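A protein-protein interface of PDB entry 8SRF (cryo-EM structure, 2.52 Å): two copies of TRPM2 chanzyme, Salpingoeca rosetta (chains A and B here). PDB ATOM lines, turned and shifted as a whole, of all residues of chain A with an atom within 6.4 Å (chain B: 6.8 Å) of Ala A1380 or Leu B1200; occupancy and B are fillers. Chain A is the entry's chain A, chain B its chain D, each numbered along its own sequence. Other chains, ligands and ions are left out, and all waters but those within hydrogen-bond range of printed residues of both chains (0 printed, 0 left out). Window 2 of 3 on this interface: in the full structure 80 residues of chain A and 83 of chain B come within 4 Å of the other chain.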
ATOM      1  N   ASP A1378     -18.592  28.666   2.347  1.00  0.00           N
ATOM      2  CA  ASP A1378     -19.116  28.241   1.060  1.00  0.00           C
ATOM      3  C   ASP A1378     -18.022  27.434   0.354  1.00  0.00           C
ATOM      4  O   ASP A1378     -16.947  27.230   0.914  1.00  0.00           O
ATOM      5  CB  ASP A1378     -19.555  29.472   0.254  1.00  0.00           C
ATOM      6  CG  ASP A1378     -20.677  29.177  -0.736  1.00  0.00           C
ATOM      7  OD1 ASP A1378     -21.580  28.387  -0.392  1.00  0.00           O
ATOM      8  OD2 ASP A1378     -20.645  29.732  -1.854  1.00  0.00           O
ATOM      9  N   VAL A1379     -18.325  26.923  -0.851  1.00  0.00           N
ATOM     10  CA  VAL A1379     -17.387  26.099  -1.623  1.00  0.00           C
ATOM     11  C   VAL A1379     -16.201  26.924  -2.156  1.00  0.00           C
ATOM     12  O   VAL A1379     -15.073  26.406  -2.254  1.00  0.00           O
ATOM     13  CB  VAL A1379     -18.210  25.404  -2.738  1.00  0.00           C
ATOM     14  CG1 VAL A1379     -17.410  24.469  -3.661  1.00  0.00           C
ATOM     15  CG2 VAL A1379     -19.387  24.650  -2.117  1.00  0.00           C
ATOM     16  N   ALA A1380     -16.451  28.218  -2.468  1.00  0.00           N
ATOM     17  CA  ALA A1380     -15.476  29.196  -2.993  1.00  0.00           C
ATOM     18  C   ALA A1380     -14.289  29.433  -2.060  1.00  0.00           C
ATOM     19  O   ALA A1380     -13.117  29.257  -2.453  1.00  0.00           O
ATOM     20  CB  ALA A1380     -16.180  30.521  -3.277  1.00  0.00           C
ATOM     21  N   LEU A1381     -14.618  29.755  -0.795  1.00  0.00           N
ATOM     22  CA  LEU A1381     -13.657  29.990   0.278  1.00  0.00           C
ATOM     23  C   LEU A1381     -12.921  28.712   0.641  1.00  0.00           C
ATOM     24  O   LEU A1381     -11.728  28.780   0.965  1.00  0.00           O
ATOM     25  CB  LEU A1381     -14.376  30.625   1.469  1.00  0.00           C
ATOM     26  CG  LEU A1381     -13.708  30.932   2.803  1.00  0.00           C
ATOM     27  CD1 LEU A1381     -12.489  31.756   2.626  1.00  0.00           C
ATOM     28  CD2 LEU A1381     -14.694  31.790   3.551  1.00  0.00           C
ATOM     29  N   THR A1382     -13.652  27.572   0.682  1.00  0.00           N
ATOM     30  CA  THR A1382     -13.113  26.275   1.108  1.00  0.00           C
ATOM     31  C   THR A1382     -12.075  25.788   0.104  1.00  0.00           C
ATOM     32  O   THR A1382     -10.985  25.362   0.504  1.00  0.00           O
ATOM     33  CB  THR A1382     -14.228  25.240   1.251  1.00  0.00           C
ATOM     34  OG1 THR A1382     -15.270  25.773   2.077  1.00  0.00           O
ATOM     35  CG2 THR A1382     -13.718  23.947   1.855  1.00  0.00           C
ATOM     36  N   SER A1383     -12.417  25.906  -1.202  1.00  0.00           N
ATOM     37  CA  SER A1383     -11.594  25.503  -2.351  1.00  0.00           C
ATOM     38  C   SER A1383     -10.296  26.299  -2.394  1.00  0.00           C
ATOM     39  O   SER A1383      -9.201  25.711  -2.508  1.00  0.00           O
ATOM     40  CB  SER A1383     -12.378  25.685  -3.649  1.00  0.00           C
ATOM     41  OG  SER A1383     -13.509  24.836  -3.680  1.00  0.00           O
ATOM     42  N   GLY A1384     -10.437  27.643  -2.302  1.00  0.00           N
ATOM     43  CA  GLY A1384      -9.292  28.549  -2.281  1.00  0.00           C
ATOM     44  C   GLY A1384      -8.399  28.370  -1.062  1.00  0.00           C
ATOM     45  O   GLY A1384      -7.170  28.343  -1.196  1.00  0.00           O
ATOM     46  N   ARG A1385      -9.022  28.261   0.137  1.00  0.00           N
ATOM     47  CA  ARG A1385      -8.330  28.103   1.420  1.00  0.00           C
ATOM     48  C   ARG A1385      -7.551  26.790   1.508  1.00  0.00           C
ATOM     49  O   ARG A1385      -6.402  26.793   1.962  1.00  0.00           O
ATOM     50  CB  ARG A1385      -9.344  28.215   2.561  1.00  0.00           C
ATOM     51  CG  ARG A1385      -8.755  28.142   3.960  1.00  0.00           C
ATOM     52  CD  ARG A1385      -9.841  28.178   5.029  1.00  0.00           C
ATOM     53  NE  ARG A1385     -10.980  27.319   4.723  1.00  0.00           N
ATOM     54  CZ  ARG A1385     -11.049  26.015   4.966  1.00  0.00           C
ATOM     55  NH1 ARG A1385     -10.046  25.355   5.522  1.00  0.00           N
ATOM     56  NH2 ARG A1385     -12.158  25.357   4.649  1.00  0.00           N
ATOM     57  N   PHE A1413      -7.930  32.705  -9.641  1.00  0.00           N
ATOM     58  CA  PHE A1413      -9.060  32.173  -8.882  1.00  0.00           C
ATOM     59  C   PHE A1413     -10.387  32.834  -9.223  1.00  0.00           C
ATOM     60  O   PHE A1413     -11.421  32.405  -8.699  1.00  0.00           O
ATOM     61  CB  PHE A1413      -8.817  32.342  -7.372  1.00  0.00           C
ATOM     62  CG  PHE A1413      -7.964  31.263  -6.715  1.00  0.00           C
ATOM     63  CD1 PHE A1413      -7.210  30.322  -7.455  1.00  0.00           C
ATOM     64  CD2 PHE A1413      -7.885  31.249  -5.313  1.00  0.00           C
ATOM     65  CE1 PHE A1413      -6.428  29.362  -6.803  1.00  0.00           C
ATOM     66  CE2 PHE A1413      -7.099  30.305  -4.648  1.00  0.00           C
ATOM     67  CZ  PHE A1413      -6.380  29.364  -5.398  1.00  0.00           C
ATOM     68  N   SER A1414     -10.393  33.854 -10.081  1.00  0.00           N
ATOM     69  CA  SER A1414     -11.633  34.543 -10.411  1.00  0.00           C
ATOM     70  C   SER A1414     -12.459  33.826 -11.472  1.00  0.00           C
ATOM     71  O   SER A1414     -13.634  34.160 -11.645  1.00  0.00           O
ATOM     72  CB  SER A1414     -11.328  35.965 -10.878  1.00  0.00           C
ATOM     73  OG  SER A1414     -10.404  35.958 -11.950  1.00  0.00           O
ATOM     74  N   SER A1415     -11.890  32.852 -12.179  1.00  0.00           N
ATOM     75  CA  SER A1415     -12.604  32.145 -13.236  1.00  0.00           C
ATOM     76  C   SER A1415     -12.567  30.649 -12.967  1.00  0.00           C
ATOM     77  O   SER A1415     -11.670  29.953 -13.451  1.00  0.00           O
ATOM     78  CB  SER A1415     -12.001  32.454 -14.608  1.00  0.00           C
ATOM     79  OG  SER A1415     -12.719  31.800 -15.639  1.00  0.00           O
ATOM     80  N   GLY A1416     -13.538  30.160 -12.202  1.00  0.00           N
ATOM     81  CA  GLY A1416     -13.629  28.743 -11.905  1.00  0.00           C
ATOM     82  C   GLY A1416     -14.975  28.182 -12.299  1.00  0.00           C
ATOM     83  O   GLY A1416     -16.012  28.836 -12.148  1.00  0.00           O
ATOM     84  N   THR A1417     -14.949  26.951 -12.803  1.00  0.00           N
ATOM     85  CA  THR A1417     -16.155  26.268 -13.249  1.00  0.00           C
ATOM     86  C   THR A1417     -16.328  25.005 -12.419  1.00  0.00           C
ATOM     87  O   THR A1417     -15.389  24.212 -12.297  1.00  0.00           O
ATOM     88  CB  THR A1417     -16.047  25.935 -14.748  1.00  0.00           C
ATOM     89  OG1 THR A1417     -15.878  27.149 -15.491  1.00  0.00           O
ATOM     90  CG2 THR A1417     -17.290  25.224 -15.268  1.00  0.00           C
ATOM     91  N   ILE A1418     -17.513  24.831 -11.833  1.00  0.00           N
ATOM     92  CA  ILE A1418     -17.847  23.625 -11.078  1.00  0.00           C
ATOM     93  C   ILE A1418     -18.120  22.523 -12.101  1.00  0.00           C
ATOM     94  O   ILE A1418     -19.092  22.588 -12.859  1.00  0.00           O
ATOM     95  CB  ILE A1418     -19.036  23.849 -10.141  1.00  0.00           C
ATOM     96  CG1 ILE A1418     -18.633  24.822  -9.029  1.00  0.00           C
ATOM     97  CG2 ILE A1418     -19.474  22.525  -9.503  1.00  0.00           C
ATOM     98  CD1 ILE A1418     -19.741  25.175  -8.043  1.00  0.00           C
ATOM     99  N   VAL A1440     -14.020  21.958  -8.281  1.00  0.00           N
ATOM    100  CA  VAL A1440     -13.880  23.272  -8.899  1.00  0.00           C
ATOM    101  C   VAL A1440     -12.593  23.270  -9.705  1.00  0.00           C
ATOM    102  O   VAL A1440     -11.515  22.978  -9.169  1.00  0.00           O
ATOM    103  CB  VAL A1440     -13.849  24.412  -7.863  1.00  0.00           C
ATOM    104  CG1 VAL A1440     -14.022  25.746  -8.556  1.00  0.00           C
ATOM    105  CG2 VAL A1440     -14.914  24.249  -6.780  1.00  0.00           C
ATOM    106  N   PHE A1442      -9.874  25.317 -11.910  1.00  0.00           N
ATOM    107  CA  PHE A1442      -9.269  26.608 -12.237  1.00  0.00           C
ATOM    108  C   PHE A1442      -8.274  26.362 -13.360  1.00  0.00           C
ATOM    109  O   PHE A1442      -7.187  25.829 -13.135  1.00  0.00           O
ATOM    110  CB  PHE A1442      -8.603  27.244 -11.024  1.00  0.00           C
ATOM    111  CG  PHE A1442      -9.555  27.609  -9.929  1.00  0.00           C
ATOM    112  CD1 PHE A1442     -10.422  28.702 -10.081  1.00  0.00           C
ATOM    113  CD2 PHE A1442      -9.599  26.853  -8.761  1.00  0.00           C
ATOM    114  CE1 PHE A1442     -11.319  29.055  -9.052  1.00  0.00           C
ATOM    115  CE2 PHE A1442     -10.490  27.179  -7.720  1.00  0.00           C
ATOM    116  CZ  PHE A1442     -11.351  28.283  -7.874  1.00  0.00           C
ATOM    117  N   PRO B1196     -22.195  34.284 -16.575  1.00  0.00           N
ATOM    118  CA  PRO B1196     -22.579  34.420 -15.166  1.00  0.00           C
ATOM    119  C   PRO B1196     -23.075  33.107 -14.564  1.00  0.00           C
ATOM    120  O   PRO B1196     -23.139  32.975 -13.342  1.00  0.00           O
ATOM    121  CB  PRO B1196     -23.701  35.461 -15.211  1.00  0.00           C
ATOM    122  N   ASN B1198     -22.519  28.953 -14.178  1.00  0.00           N
ATOM    123  CA  ASN B1198     -21.314  28.167 -13.854  1.00  0.00           C
ATOM    124  C   ASN B1198     -20.061  29.036 -13.765  1.00  0.00           C
ATOM    125  O   ASN B1198     -19.121  28.867 -14.547  1.00  0.00           O
ATOM    126  CB  ASN B1198     -21.094  26.998 -14.828  1.00  0.00           C
ATOM    127  N   ARG B1199     -20.050  29.954 -12.804  1.00  0.00           N
ATOM    128  CA  ARG B1199     -18.941  30.876 -12.591  1.00  0.00           C
ATOM    129  C   ARG B1199     -18.765  31.120 -11.101  1.00  0.00           C
ATOM    130  O   ARG B1199     -19.710  31.492 -10.401  1.00  0.00           O
ATOM    131  CB  ARG B1199     -19.169  32.215 -13.306  1.00  0.00           C
ATOM    132  CG  ARG B1199     -18.810  32.243 -14.790  1.00  0.00           C
ATOM    133  CD  ARG B1199     -17.297  32.474 -14.984  1.00  0.00           C
ATOM    134  NE  ARG B1199     -16.830  32.466 -16.372  1.00  0.00           N
ATOM    135  CZ  ARG B1199     -16.662  31.397 -17.148  1.00  0.00           C
ATOM    136  NH1 ARG B1199     -16.878  30.165 -16.711  1.00  0.00           N
ATOM    137  NH2 ARG B1199     -16.253  31.571 -18.402  1.00  0.00           N
ATOM    138  N   LEU B1200     -17.547  30.910 -10.613  1.00  0.00           N
ATOM    139  CA  LEU B1200     -17.294  30.972  -9.183  1.00  0.00           C
ATOM    140  C   LEU B1200     -16.077  31.858  -8.970  1.00  0.00           C
ATOM    141  O   LEU B1200     -15.091  31.762  -9.704  1.00  0.00           O
ATOM    142  CB  LEU B1200     -17.069  29.565  -8.615  1.00  0.00           C
ATOM    143  CG  LEU B1200     -16.908  29.405  -7.108  1.00  0.00           C
ATOM    144  CD1 LEU B1200     -18.201  29.842  -6.444  1.00  0.00           C
ATOM    145  CD2 LEU B1200     -16.577  27.971  -6.752  1.00  0.00           C
ATOM    146  N   ASN B1201     -16.158  32.712  -7.954  1.00  0.00           N
ATOM    147  CA  ASN B1201     -15.114  33.656  -7.590  1.00  0.00           C
ATOM    148  C   ASN B1201     -14.542  33.273  -6.232  1.00  0.00           C
ATOM    149  O   ASN B1201     -15.228  33.356  -5.208  1.00  0.00           O
ATOM    150  CB  ASN B1201     -15.672  35.086  -7.553  1.00  0.00           C
ATOM    151  CG  ASN B1201     -14.587  36.161  -7.616  1.00  0.00           C
ATOM    152  OD1 ASN B1201     -13.391  35.873  -7.681  1.00  0.00           O
ATOM    153  ND2 ASN B1201     -15.015  37.418  -7.593  1.00  0.00           N
ATOM    154  N   SER B1202     -13.274  32.857  -6.238  1.00  0.00           N
ATOM    155  CA  SER B1202     -12.582  32.405  -5.037  1.00  0.00           C
ATOM    156  C   SER B1202     -11.572  33.434  -4.545  1.00  0.00           C
ATOM    157  O   SER B1202     -10.657  33.084  -3.792  1.00  0.00           O
ATOM    158  CB  SER B1202     -11.890  31.063  -5.281  1.00  0.00           C
ATOM    159  OG  SER B1202     -12.837  30.017  -5.398  1.00  0.00           O
ATOM    160  N   ALA B1203     -11.709  34.697  -4.982  1.00  0.00           N
ATOM    161  CA  ALA B1203     -10.840  35.796  -4.555  1.00  0.00           C
ATOM    162  C   ALA B1203     -11.027  36.191  -3.086  1.00  0.00           C
ATOM    163  O   ALA B1203     -10.135  36.853  -2.530  1.00  0.00           O
ATOM    164  CB  ALA B1203     -11.067  37.019  -5.443  1.00  0.00           C
ATOM    165  N   VAL B1204     -12.193  35.871  -2.486  1.00  0.00           N
ATOM    166  CA  VAL B1204     -12.516  36.127  -1.075  1.00  0.00           C
ATOM    167  C   VAL B1204     -11.567  35.360  -0.125  1.00  0.00           C
ATOM    168  O   VAL B1204     -11.243  35.852   0.967  1.00  0.00           O
ATOM    169  CB  VAL B1204     -14.030  35.836  -0.867  1.00  0.00           C
ATOM    170  CG1 VAL B1204     -14.433  34.409  -1.275  1.00  0.00           C
ATOM    171  CG2 VAL B1204     -14.560  36.224   0.531  1.00  0.00           C
ATOM    172  N   ALA B1205     -11.063  34.175  -0.548  1.00  0.00           N
ATOM    173  CA  ALA B1205     -10.065  33.388   0.188  1.00  0.00           C
ATOM    174  C   ALA B1205      -8.701  34.077   0.246  1.00  0.00           C
ATOM    175  O   ALA B1205      -7.913  33.826   1.165  1.00  0.00           O
ATOM    176  CB  ALA B1205      -9.925  32.003  -0.440  1.00  0.00           C
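The backbone carbonyl oxygen of Ala A1380 sits at hydrogen-bond distance from the side-chain hydroxyl of Ser B1202.
O of Phe A1413 lies within hydrogen-bond range of N of Ser B1202.
O of Gly A1416 sits at hydrogen-bond distance from N of Leu B1200.
The side-chain hydroxyl (OG1) of Thr A1417 lies within hydrogen-bond range of the guanidinium group (NH1) of Arg B1199 (3.4 Å).
O of Ser A1414 sits close to O of Leu B1200 (3.4 Å).
OD1 of Asn B1201 is in hydrogen-bond range of N of Ala B1203, at 3.4 Å.
Ala A1380 touches Leu B1200.
Asn B1201 touches Ala A1380 (O to CB, 3.6 Å).
Leu A1381 touches Ala B1205.
Gly A1384 touches Ala B1205 (CA to CB, 3.96 Å).
Ala B1205 touches Arg A1385 (CB to N, 3.9 Å).
Asn B1201 touches Ser A1414 (OD1 to CA, 3.5 Å).
Gly A1416 touches Asn B1198.
CA of Arg B1199 touches O of Gly A1416, 3.6 Å away.
Asn B1198 touches Thr A1417.
OG of Ser B1202 touches CZ of Phe A1442 (3.4 Å).
Val A1379 touches none of the printed residues of chain B.
Of chain B, only Leu B1200 (3.8 Å), Asn B1201 (3.6 Å) and Ser B1202 (3.1 Å) come within 4 Å of Ala A1380.
Printed residues of chain B within 4 Å of Gly A1384: Ala B1205.
Of the printed residues of chain A, Ala B1205 touches Leu A1381 (3.8 Å), Gly A1384 (3.96 Å) and Arg A1385 (3.9 Å).
The nearest residue of chain B that does not touch Ala A1380 is Ala B1205 (4.7 Å).
The nearest residue of chain A that does not touch Leu B1200 is Ser A1415 (4.2 Å).
The nearest printed residue of chain A that does not touch Arg B1199 is Ser A1415 (4.2 Å).
Among the printed residues, 17 pairs touch across the chains.
Among the printed residues, no Asp or Glu carboxylate lies within 4 Å of a Lys or Arg side-chain nitrogen of the other chain.
No position is printed for both chains.
Of the 17 pairs that touch across the chains among the printed residues, none has its exchanged pair printed and touching as well.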
